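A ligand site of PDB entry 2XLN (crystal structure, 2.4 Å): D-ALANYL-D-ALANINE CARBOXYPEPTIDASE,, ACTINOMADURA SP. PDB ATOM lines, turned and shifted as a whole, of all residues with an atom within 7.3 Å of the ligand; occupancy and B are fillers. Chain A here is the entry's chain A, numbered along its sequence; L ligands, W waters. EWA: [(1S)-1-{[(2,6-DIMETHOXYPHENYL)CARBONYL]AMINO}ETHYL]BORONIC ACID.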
ATOM      1  N   PRO A  47      21.469  12.149  27.233  1.00  0.00           N
ATOM      2  CA  PRO A  47      21.257  13.051  26.089  1.00  0.00           C
ATOM      3  C   PRO A  47      19.897  12.887  25.401  1.00  0.00           C
ATOM      4  O   PRO A  47      19.464  13.768  24.670  1.00  0.00           O
ATOM      5  CB  PRO A  47      22.362  12.644  25.113  1.00  0.00           C
ATOM      6  CG  PRO A  47      22.636  11.198  25.433  1.00  0.00           C
ATOM      7  CD  PRO A  47      22.112  10.883  26.813  1.00  0.00           C
ATOM      8  N   ALA A  48      19.238  11.752  25.663  1.00  0.00           N
ATOM      9  CA  ALA A  48      18.150  11.253  24.798  1.00  0.00           C
ATOM     10  C   ALA A  48      18.576  11.374  23.332  1.00  0.00           C
ATOM     11  O   ALA A  48      19.684  10.930  22.976  1.00  0.00           O
ATOM     12  CB  ALA A  48      16.834  11.998  25.085  1.00  0.00           C
ATOM     13  N   SER A  49      17.745  11.996  22.497  1.00  0.00           N
ATOM     14  CA  SER A  49      18.010  12.078  21.060  1.00  0.00           C
ATOM     15  C   SER A  49      19.162  12.969  20.606  1.00  0.00           C
ATOM     16  O   SER A  49      19.527  12.945  19.422  1.00  0.00           O
ATOM     17  CB  SER A  49      16.728  12.412  20.302  1.00  0.00           C
ATOM     18  OG  SER A  49      16.012  11.231  20.035  1.00  0.00           O
ATOM     19  N   ASN A  50      19.737  13.759  21.513  1.00  0.00           N
ATOM     20  CA  ASN A  50      21.024  14.426  21.254  1.00  0.00           C
ATOM     21  C   ASN A  50      22.186  13.452  20.962  1.00  0.00           C
ATOM     22  O   ASN A  50      23.209  13.854  20.397  1.00  0.00           O
ATOM     23  CB  ASN A  50      21.415  15.370  22.394  1.00  0.00           C
ATOM     24  CG  ASN A  50      20.829  16.750  22.233  1.00  0.00           C
ATOM     25  OD1 ASN A  50      19.769  16.916  21.636  1.00  0.00           O
ATOM     26  ND2 ASN A  50      21.511  17.758  22.766  1.00  0.00           N
ATOM     27  N   LYS A  52      22.024  11.302  18.703  1.00  0.00           N
ATOM     28  CA  LYS A  52      22.019  11.247  17.244  1.00  0.00           C
ATOM     29  C   LYS A  52      23.016  12.208  16.616  1.00  0.00           C
ATOM     30  O   LYS A  52      23.499  11.958  15.511  1.00  0.00           O
ATOM     31  CB  LYS A  52      20.624  11.536  16.686  1.00  0.00           C
ATOM     32  CG  LYS A  52      19.678  10.368  16.706  1.00  0.00           C
ATOM     33  CD  LYS A  52      18.278  10.808  16.309  1.00  0.00           C
ATOM     34  CE  LYS A  52      17.275   9.690  16.445  1.00  0.00           C
ATOM     35  NZ  LYS A  52      16.829   9.450  17.867  1.00  0.00           N
ATOM     36  N   ASP A 142       7.936  -0.319  25.822  1.00  0.00           N
ATOM     37  CA  ASP A 142       8.110   0.564  24.660  1.00  0.00           C
ATOM     38  C   ASP A 142       7.911  -0.160  23.316  1.00  0.00           C
ATOM     39  O   ASP A 142       7.610   0.465  22.296  1.00  0.00           O
ATOM     40  CB  ASP A 142       9.502   1.204  24.670  1.00  0.00           C
ATOM     41  CG  ASP A 142       9.602   2.401  25.617  1.00  0.00           C
ATOM     42  OD1 ASP A 142       8.618   2.751  26.308  1.00  0.00           O
ATOM     43  OD2 ASP A 142      10.700   3.011  25.650  1.00  0.00           O
ATOM     44  N   ALA A 146       6.597   2.872  17.520  1.00  0.00           N
ATOM     45  CA  ALA A 146       7.497   3.086  16.377  1.00  0.00           C
ATOM     46  C   ALA A 146       8.937   3.407  16.757  1.00  0.00           C
ATOM     47  O   ALA A 146       9.861   3.034  16.044  1.00  0.00           O
ATOM     48  CB  ALA A 146       6.961   4.173  15.450  1.00  0.00           C
ATOM     49  N   TYR A 147       9.112   4.100  17.884  1.00  0.00           N
ATOM     50  CA  TYR A 147      10.449   4.506  18.334  1.00  0.00           C
ATOM     51  C   TYR A 147      11.238   3.370  18.967  1.00  0.00           C
ATOM     52  O   TYR A 147      12.410   3.539  19.289  1.00  0.00           O
ATOM     53  CB  TYR A 147      10.385   5.714  19.277  1.00  0.00           C
ATOM     54  CG  TYR A 147       9.403   5.582  20.430  1.00  0.00           C
ATOM     55  CD1 TYR A 147       9.766   4.924  21.613  1.00  0.00           C
ATOM     56  CD2 TYR A 147       8.134   6.151  20.350  1.00  0.00           C
ATOM     57  CE1 TYR A 147       8.868   4.814  22.676  1.00  0.00           C
ATOM     58  CE2 TYR A 147       7.236   6.057  21.398  1.00  0.00           C
ATOM     59  CZ  TYR A 147       7.599   5.385  22.560  1.00  0.00           C
ATOM     60  OH  TYR A 147       6.686   5.293  23.591  1.00  0.00           O
ATOM     61  N   SER A 148      10.578   2.214  19.144  1.00  0.00           N
ATOM     62  CA  SER A 148      11.216   0.996  19.667  1.00  0.00           C
ATOM     63  C   SER A 148      11.067  -0.177  18.682  1.00  0.00           C
ATOM     64  O   SER A 148      10.954  -1.350  19.087  1.00  0.00           O
ATOM     65  CB  SER A 148      10.621   0.627  21.026  1.00  0.00           C
ATOM     66  OG  SER A 148      11.327  -0.463  21.599  1.00  0.00           O
ATOM     67  N   LYS A 296      15.559  15.377  11.376  1.00  0.00           N
ATOM     68  CA  LYS A 296      14.458  16.342  11.535  1.00  0.00           C
ATOM     69  C   LYS A 296      13.391  15.813  12.483  1.00  0.00           C
ATOM     70  O   LYS A 296      12.907  16.538  13.357  1.00  0.00           O
ATOM     71  CB  LYS A 296      13.807  16.692  10.181  1.00  0.00           C
ATOM     72  CG  LYS A 296      14.697  17.461   9.202  1.00  0.00           C
ATOM     73  CD  LYS A 296      14.981  18.897   9.627  1.00  0.00           C
ATOM     74  CE  LYS A 296      15.655  19.640   8.487  1.00  0.00           C
ATOM     75  NZ  LYS A 296      15.942  21.069   8.784  1.00  0.00           N
ATOM     76  N   PHE A 297      13.055  14.540  12.295  1.00  0.00           N
ATOM     77  CA  PHE A 297      11.988  13.868  13.054  1.00  0.00           C
ATOM     78  C   PHE A 297      12.528  12.925  14.107  1.00  0.00           C
ATOM     79  O   PHE A 297      11.753  12.301  14.842  1.00  0.00           O
ATOM     80  CB  PHE A 297      11.044  13.130  12.101  1.00  0.00           C
ATOM     81  CG  PHE A 297      10.547  13.965  10.955  1.00  0.00           C
ATOM     82  CD1 PHE A 297       9.745  15.077  11.191  1.00  0.00           C
ATOM     83  CD2 PHE A 297      10.897  13.638   9.636  1.00  0.00           C
ATOM     84  CE1 PHE A 297       9.290  15.863  10.135  1.00  0.00           C
ATOM     85  CE2 PHE A 297      10.447  14.418   8.573  1.00  0.00           C
ATOM     86  CZ  PHE A 297       9.644  15.531   8.823  1.00  0.00           C
ATOM     87  N   SER A 298      13.856  12.811  14.188  1.00  0.00           N
ATOM     88  CA  SER A 298      14.511  12.050  15.252  1.00  0.00           C
ATOM     89  C   SER A 298      14.169  10.549  15.138  1.00  0.00           C
ATOM     90  O   SER A 298      13.534   9.969  16.042  1.00  0.00           O
ATOM     91  CB  SER A 298      14.118  12.646  16.616  1.00  0.00           C
ATOM     92  OG  SER A 298      14.995  12.261  17.647  1.00  0.00           O
ATOM     93  N   ASN A 299      14.586   9.953  14.022  1.00  0.00           N
ATOM     94  CA  ASN A 299      14.303   8.535  13.717  1.00  0.00           C
ATOM     95  C   ASN A 299      15.268   7.572  14.413  1.00  0.00           C
ATOM     96  O   ASN A 299      16.454   7.505  14.068  1.00  0.00           O
ATOM     97  CB  ASN A 299      14.330   8.308  12.197  1.00  0.00           C
ATOM     98  CG  ASN A 299      13.573   7.025  11.781  1.00  0.00           C
ATOM     99  OD1 ASN A 299      12.607   7.094  11.012  1.00  0.00           O
ATOM    100  ND2 ASN A 299      14.011   5.885  12.268  1.00  0.00           N
ATOM    101  N   ASN A 300      14.742   6.821  15.368  1.00  0.00           N
ATOM    102  CA  ASN A 300      15.546   5.885  16.166  1.00  0.00           C
ATOM    103  C   ASN A 300      16.067   4.718  15.340  1.00  0.00           C
ATOM    104  O   ASN A 300      17.225   4.330  15.460  1.00  0.00           O
ATOM    105  CB  ASN A 300      14.747   5.377  17.383  1.00  0.00           C
ATOM    106  CG  ASN A 300      14.612   6.415  18.501  1.00  0.00           C
ATOM    107  OD1 ASN A 300      15.222   7.483  18.459  1.00  0.00           O
ATOM    108  ND2 ASN A 300      13.829   6.078  19.520  1.00  0.00           N
ATOM    109  N   ASP A 345      23.827   3.171  22.630  1.00  0.00           N
ATOM    110  CA  ASP A 345      23.138   2.996  21.362  1.00  0.00           C
ATOM    111  C   ASP A 345      23.360   4.224  20.467  1.00  0.00           C
ATOM    112  O   ASP A 345      24.071   5.171  20.866  1.00  0.00           O
ATOM    113  CB  ASP A 345      21.643   2.673  21.562  1.00  0.00           C
ATOM    114  CG  ASP A 345      20.807   3.858  22.052  1.00  0.00           C
ATOM    115  OD1 ASP A 345      21.294   5.022  22.035  1.00  0.00           O
ATOM    116  OD2 ASP A 345      19.645   3.611  22.448  1.00  0.00           O
ATOM    117  N   SER A 347      20.609   5.960  18.837  1.00  0.00           N
ATOM    118  CA  SER A 347      19.453   6.876  18.884  1.00  0.00           C
ATOM    119  C   SER A 347      19.354   7.784  20.110  1.00  0.00           C
ATOM    120  O   SER A 347      18.844   8.895  20.024  1.00  0.00           O
ATOM    121  CB  SER A 347      18.151   6.099  18.718  1.00  0.00           C
ATOM    122  OG  SER A 347      17.893   5.276  19.842  1.00  0.00           O
ATOM    123  N   GLY A 348      19.839   7.304  21.247  1.00  0.00           N
ATOM    124  CA  GLY A 348      19.634   7.988  22.511  1.00  0.00           C
ATOM    125  C   GLY A 348      18.511   7.384  23.321  1.00  0.00           C
ATOM    126  O   GLY A 348      18.323   7.743  24.483  1.00  0.00           O
ATOM    127  N   LEU A 349      17.761   6.464  22.719  1.00  0.00           N
ATOM    128  CA  LEU A 349      16.701   5.733  23.405  1.00  0.00           C
ATOM    129  C   LEU A 349      17.183   5.100  24.719  1.00  0.00           C
ATOM    130  O   LEU A 349      16.484   5.162  25.734  1.00  0.00           O
ATOM    131  CB  LEU A 349      16.113   4.658  22.482  1.00  0.00           C
ATOM    132  CG  LEU A 349      14.687   4.165  22.692  1.00  0.00           C
ATOM    133  CD1 LEU A 349      14.352   3.111  21.662  1.00  0.00           C
ATOM    134  CD2 LEU A 349      14.474   3.591  24.068  1.00  0.00           C
ATOM    135  N   SER A 350      18.381   4.498  24.690  1.00  0.00           N
ATOM    136  CA  SER A 350      18.959   3.836  25.856  1.00  0.00           C
ATOM    137  C   SER A 350      19.280   4.825  26.967  1.00  0.00           C
ATOM    138  O   SER A 350      19.890   5.879  26.733  1.00  0.00           O
ATOM    139  CB  SER A 350      20.223   3.037  25.465  1.00  0.00           C
ATOM    140  OG  SER A 350      20.947   2.586  26.593  1.00  0.00           O
ATOM    141  N   THR A 393      11.161  18.573  14.668  1.00  0.00           N
ATOM    142  CA  THR A 393      10.784  18.635  16.076  1.00  0.00           C
ATOM    143  C   THR A 393      10.737  20.070  16.631  1.00  0.00           C
ATOM    144  O   THR A 393      10.300  20.271  17.761  1.00  0.00           O
ATOM    145  CB  THR A 393      11.713  17.754  16.932  1.00  0.00           C
ATOM    146  OG1 THR A 393      13.075  18.076  16.633  1.00  0.00           O
ATOM    147  CG2 THR A 393      11.479  16.270  16.655  1.00  0.00           C
ATOM    148  N   LYS A 410      19.213  20.296  17.491  1.00  0.00           N
ATOM    149  CA  LYS A 410      18.661  18.958  17.677  1.00  0.00           C
ATOM    150  C   LYS A 410      17.993  18.848  19.040  1.00  0.00           C
ATOM    151  O   LYS A 410      18.503  19.339  20.048  1.00  0.00           O
ATOM    152  CB  LYS A 410      19.747  17.882  17.489  1.00  0.00           C
ATOM    153  CG  LYS A 410      19.255  16.440  17.664  1.00  0.00           C
ATOM    154  CD  LYS A 410      18.435  15.950  16.480  1.00  0.00           C
ATOM    155  CE  LYS A 410      17.741  14.632  16.794  1.00  0.00           C
ATOM    156  NZ  LYS A 410      16.492  14.813  17.602  1.00  0.00           N
ATOM    157  N   THR A 411      16.833  18.199  19.052  1.00  0.00           N
ATOM    158  CA  THR A 411      16.092  17.946  20.272  1.00  0.00           C
ATOM    159  C   THR A 411      16.486  16.600  20.875  1.00  0.00           C
ATOM    160  O   THR A 411      16.997  15.716  20.197  1.00  0.00           O
ATOM    161  CB  THR A 411      14.567  17.960  20.018  1.00  0.00           C
ATOM    162  OG1 THR A 411      14.236  17.002  19.003  1.00  0.00           O
ATOM    163  CG2 THR A 411      14.099  19.341  19.580  1.00  0.00           C
ATOM    164  N   GLY A 412      16.251  16.468  22.184  1.00  0.00           N
ATOM    165  CA  GLY A 412      16.339  15.197  22.886  1.00  0.00           C
ATOM    166  C   GLY A 412      15.139  15.147  23.827  1.00  0.00           C
ATOM    167  O   GLY A 412      14.865  16.099  24.542  1.00  0.00           O
ATOM    168  N   THR A 413      14.407  14.036  23.803  1.00  0.00           N
ATOM    169  CA  THR A 413      13.139  13.929  24.523  1.00  0.00           C
ATOM    170  C   THR A 413      12.912  12.544  25.099  1.00  0.00           C
ATOM    171  O   THR A 413      12.870  11.558  24.353  1.00  0.00           O
ATOM    172  CB  THR A 413      11.938  14.276  23.610  1.00  0.00           C
ATOM    173  OG1 THR A 413      12.243  15.414  22.799  1.00  0.00           O
ATOM    174  CG2 THR A 413      10.683  14.547  24.446  1.00  0.00           C
ATOM    175  N   MET A 414      12.759  12.486  26.422  1.00  0.00           N
ATOM    176  CA  MET A 414      12.371  11.281  27.161  1.00  0.00           C
ATOM    177  C   MET A 414      11.778  11.727  28.499  1.00  0.00           C
ATOM    178  O   MET A 414      11.747  12.921  28.802  1.00  0.00           O
ATOM    179  CB  MET A 414      13.587  10.382  27.416  1.00  0.00           C
ATOM    180  CG  MET A 414      13.916   9.419  26.286  1.00  0.00           C
ATOM    181  SD  MET A 414      15.115   8.124  26.714  1.00  0.00           S
ATOM    182  CE  MET A 414      16.346   9.013  27.677  1.00  0.00           C
ATOM    183  N   SER A 415      11.304  10.762  29.300  1.00  0.00           N
ATOM    184  CA  SER A 415      10.912  11.013  30.684  1.00  0.00           C
ATOM    185  C   SER A 415      12.093  11.582  31.457  1.00  0.00           C
ATOM    186  O   SER A 415      13.174  10.995  31.466  1.00  0.00           O
ATOM    187  CB  SER A 415      10.452   9.729  31.375  1.00  0.00           C
ATOM    188  OG  SER A 415       9.040   9.722  31.563  1.00  0.00           O
ATOM    189  N   VAL A 417      14.137  13.656  30.743  1.00  0.00           N
ATOM    190  CA  VAL A 417      15.285  14.024  29.891  1.00  0.00           C
ATOM    191  C   VAL A 417      14.863  14.928  28.723  1.00  0.00           C
ATOM    192  O   VAL A 417      14.082  14.516  27.862  1.00  0.00           O
ATOM    193  CB  VAL A 417      16.037  12.788  29.313  1.00  0.00           C
ATOM    194  CG1 VAL A 417      17.262  13.232  28.503  1.00  0.00           C
ATOM    195  CG2 VAL A 417      16.439  11.811  30.413  1.00  0.00           C
HETATM  196  O6  EWA L   1      11.927   9.154  18.961  1.00  0.00           O
HETATM  197  C5  EWA L   1      11.969   9.262  20.186  1.00  0.00           C
HETATM  198  N4  EWA L   1      13.042   9.426  20.960  1.00  0.00           N
HETATM  199  C3  EWA L   1      14.424   9.644  20.643  1.00  0.00           C
HETATM  200  B   EWA L   1      14.740  11.177  20.872  1.00  0.00           B
HETATM  201  O2  EWA L   1      13.706  12.026  20.146  1.00  0.00           O
HETATM  202  O1  EWA L   1      14.650  11.526  22.366  1.00  0.00           O
HETATM  203  C16 EWA L   1      15.198   8.782  21.632  1.00  0.00           C
HETATM  204  C7  EWA L   1      10.982  10.125  20.915  1.00  0.00           C
HETATM  205  C14 EWA L   1      10.401   9.504  22.016  1.00  0.00           C
HETATM  206  O15 EWA L   1      10.873   8.179  22.422  1.00  0.00           O
HETATM  207  C15 EWA L   1      11.029   7.760  23.784  1.00  0.00           C
HETATM  208  C13 EWA L   1       9.460  10.250  22.733  1.00  0.00           C
HETATM  209  C12 EWA L   1       9.075  11.519  22.280  1.00  0.00           C
HETATM  210  C11 EWA L   1       9.627  12.072  21.130  1.00  0.00           C
HETATM  211  C8  EWA L   1      10.561  11.351  20.381  1.00  0.00           C
HETATM  212  O9  EWA L   1      11.185  11.935  19.189  1.00  0.00           O
HETATM  213  C10 EWA L   1      10.545  12.931  18.397  1.00  0.00           C
HETATM  214  O   HOH W   1      12.149   6.840  16.357  1.00  0.00           O
HETATM  215  O   HOH W   2      13.783  14.828  20.224  1.00  0.00           O
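O1 of the ligand sits close to N of Ser 49.
OG of Ser 49 is covalently linked to B of the ligand.
An oxygen (O1) of the ligand is in hydrogen-bond range of the backbone NH (N) of Thr 413 (2.9 Å).
O1 of the ligand sits at hydrogen-bond distance from O of Thr 413 (2.7 Å).
OG of Ser 298 sits at hydrogen-bond distance from O2 of the ligand (2.8 Å).
OG of Ser 49 sits at hydrogen-bond distance from OG of Ser 298 (2.8 Å).
The side-chain hydroxyl (OG) of Ser 298 is in hydrogen-bond range of the side-chain amino group (NZ) of Lys 52, at 3.4 Å.
The side-chain amino group (NZ) of Lys 410 lies within hydrogen-bond range of the side-chain hydroxyl (OG) of Ser 298, at 3.0 Å.
The side-chain amino group of Lys 52 lies within hydrogen-bond range of the side-chain amide oxygen of Asn 300, 2.6 Å away.
N of Leu 349 sits at hydrogen-bond distance from OG of Ser 347, 3.1 Å away.
OD2 of Asp 345 sits at hydrogen-bond distance from N of Leu 349 (3.4 Å).
OG1 of Thr 411 lies within hydrogen-bond range of OG1 of Thr 393, at 2.8 Å.
The side-chain carboxylate (OD1) of Asp 345 lies within hydrogen-bond range of the backbone NH (N) of Gly 348 (2.8 Å).
Residues that only touch the ligand: Asn 300 (3.2 Å), Ala 48 (3.5 Å), Tyr 147 (3.5 Å), Leu 349 (3.6 Å), Lys 52 (3.7 Å), Phe 297 (3.8 Å), Thr 393 (3.9 Å), Gly 412 (3.9 Å), Gly 348 (3.97 Å) and Ser 347 (3.99 Å).
Hydrophobic or aromatic side chains that line the ligand: Ala 48 and Tyr 147.
Water W2 lies within hydrogen-bond range of OG1 of Thr 411 (2.5 Å), O2 of the ligand (2.8 Å) and OG1 of Thr 413 (3.1 Å).
Water W1 lies within hydrogen-bond range of the backbone NH (N) of Asn 300 (2.8 Å), the backbone carbonyl oxygen (O) of Ser 298 (3.4 Å) and an oxygen (O6) of the ligand (3.5 Å).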
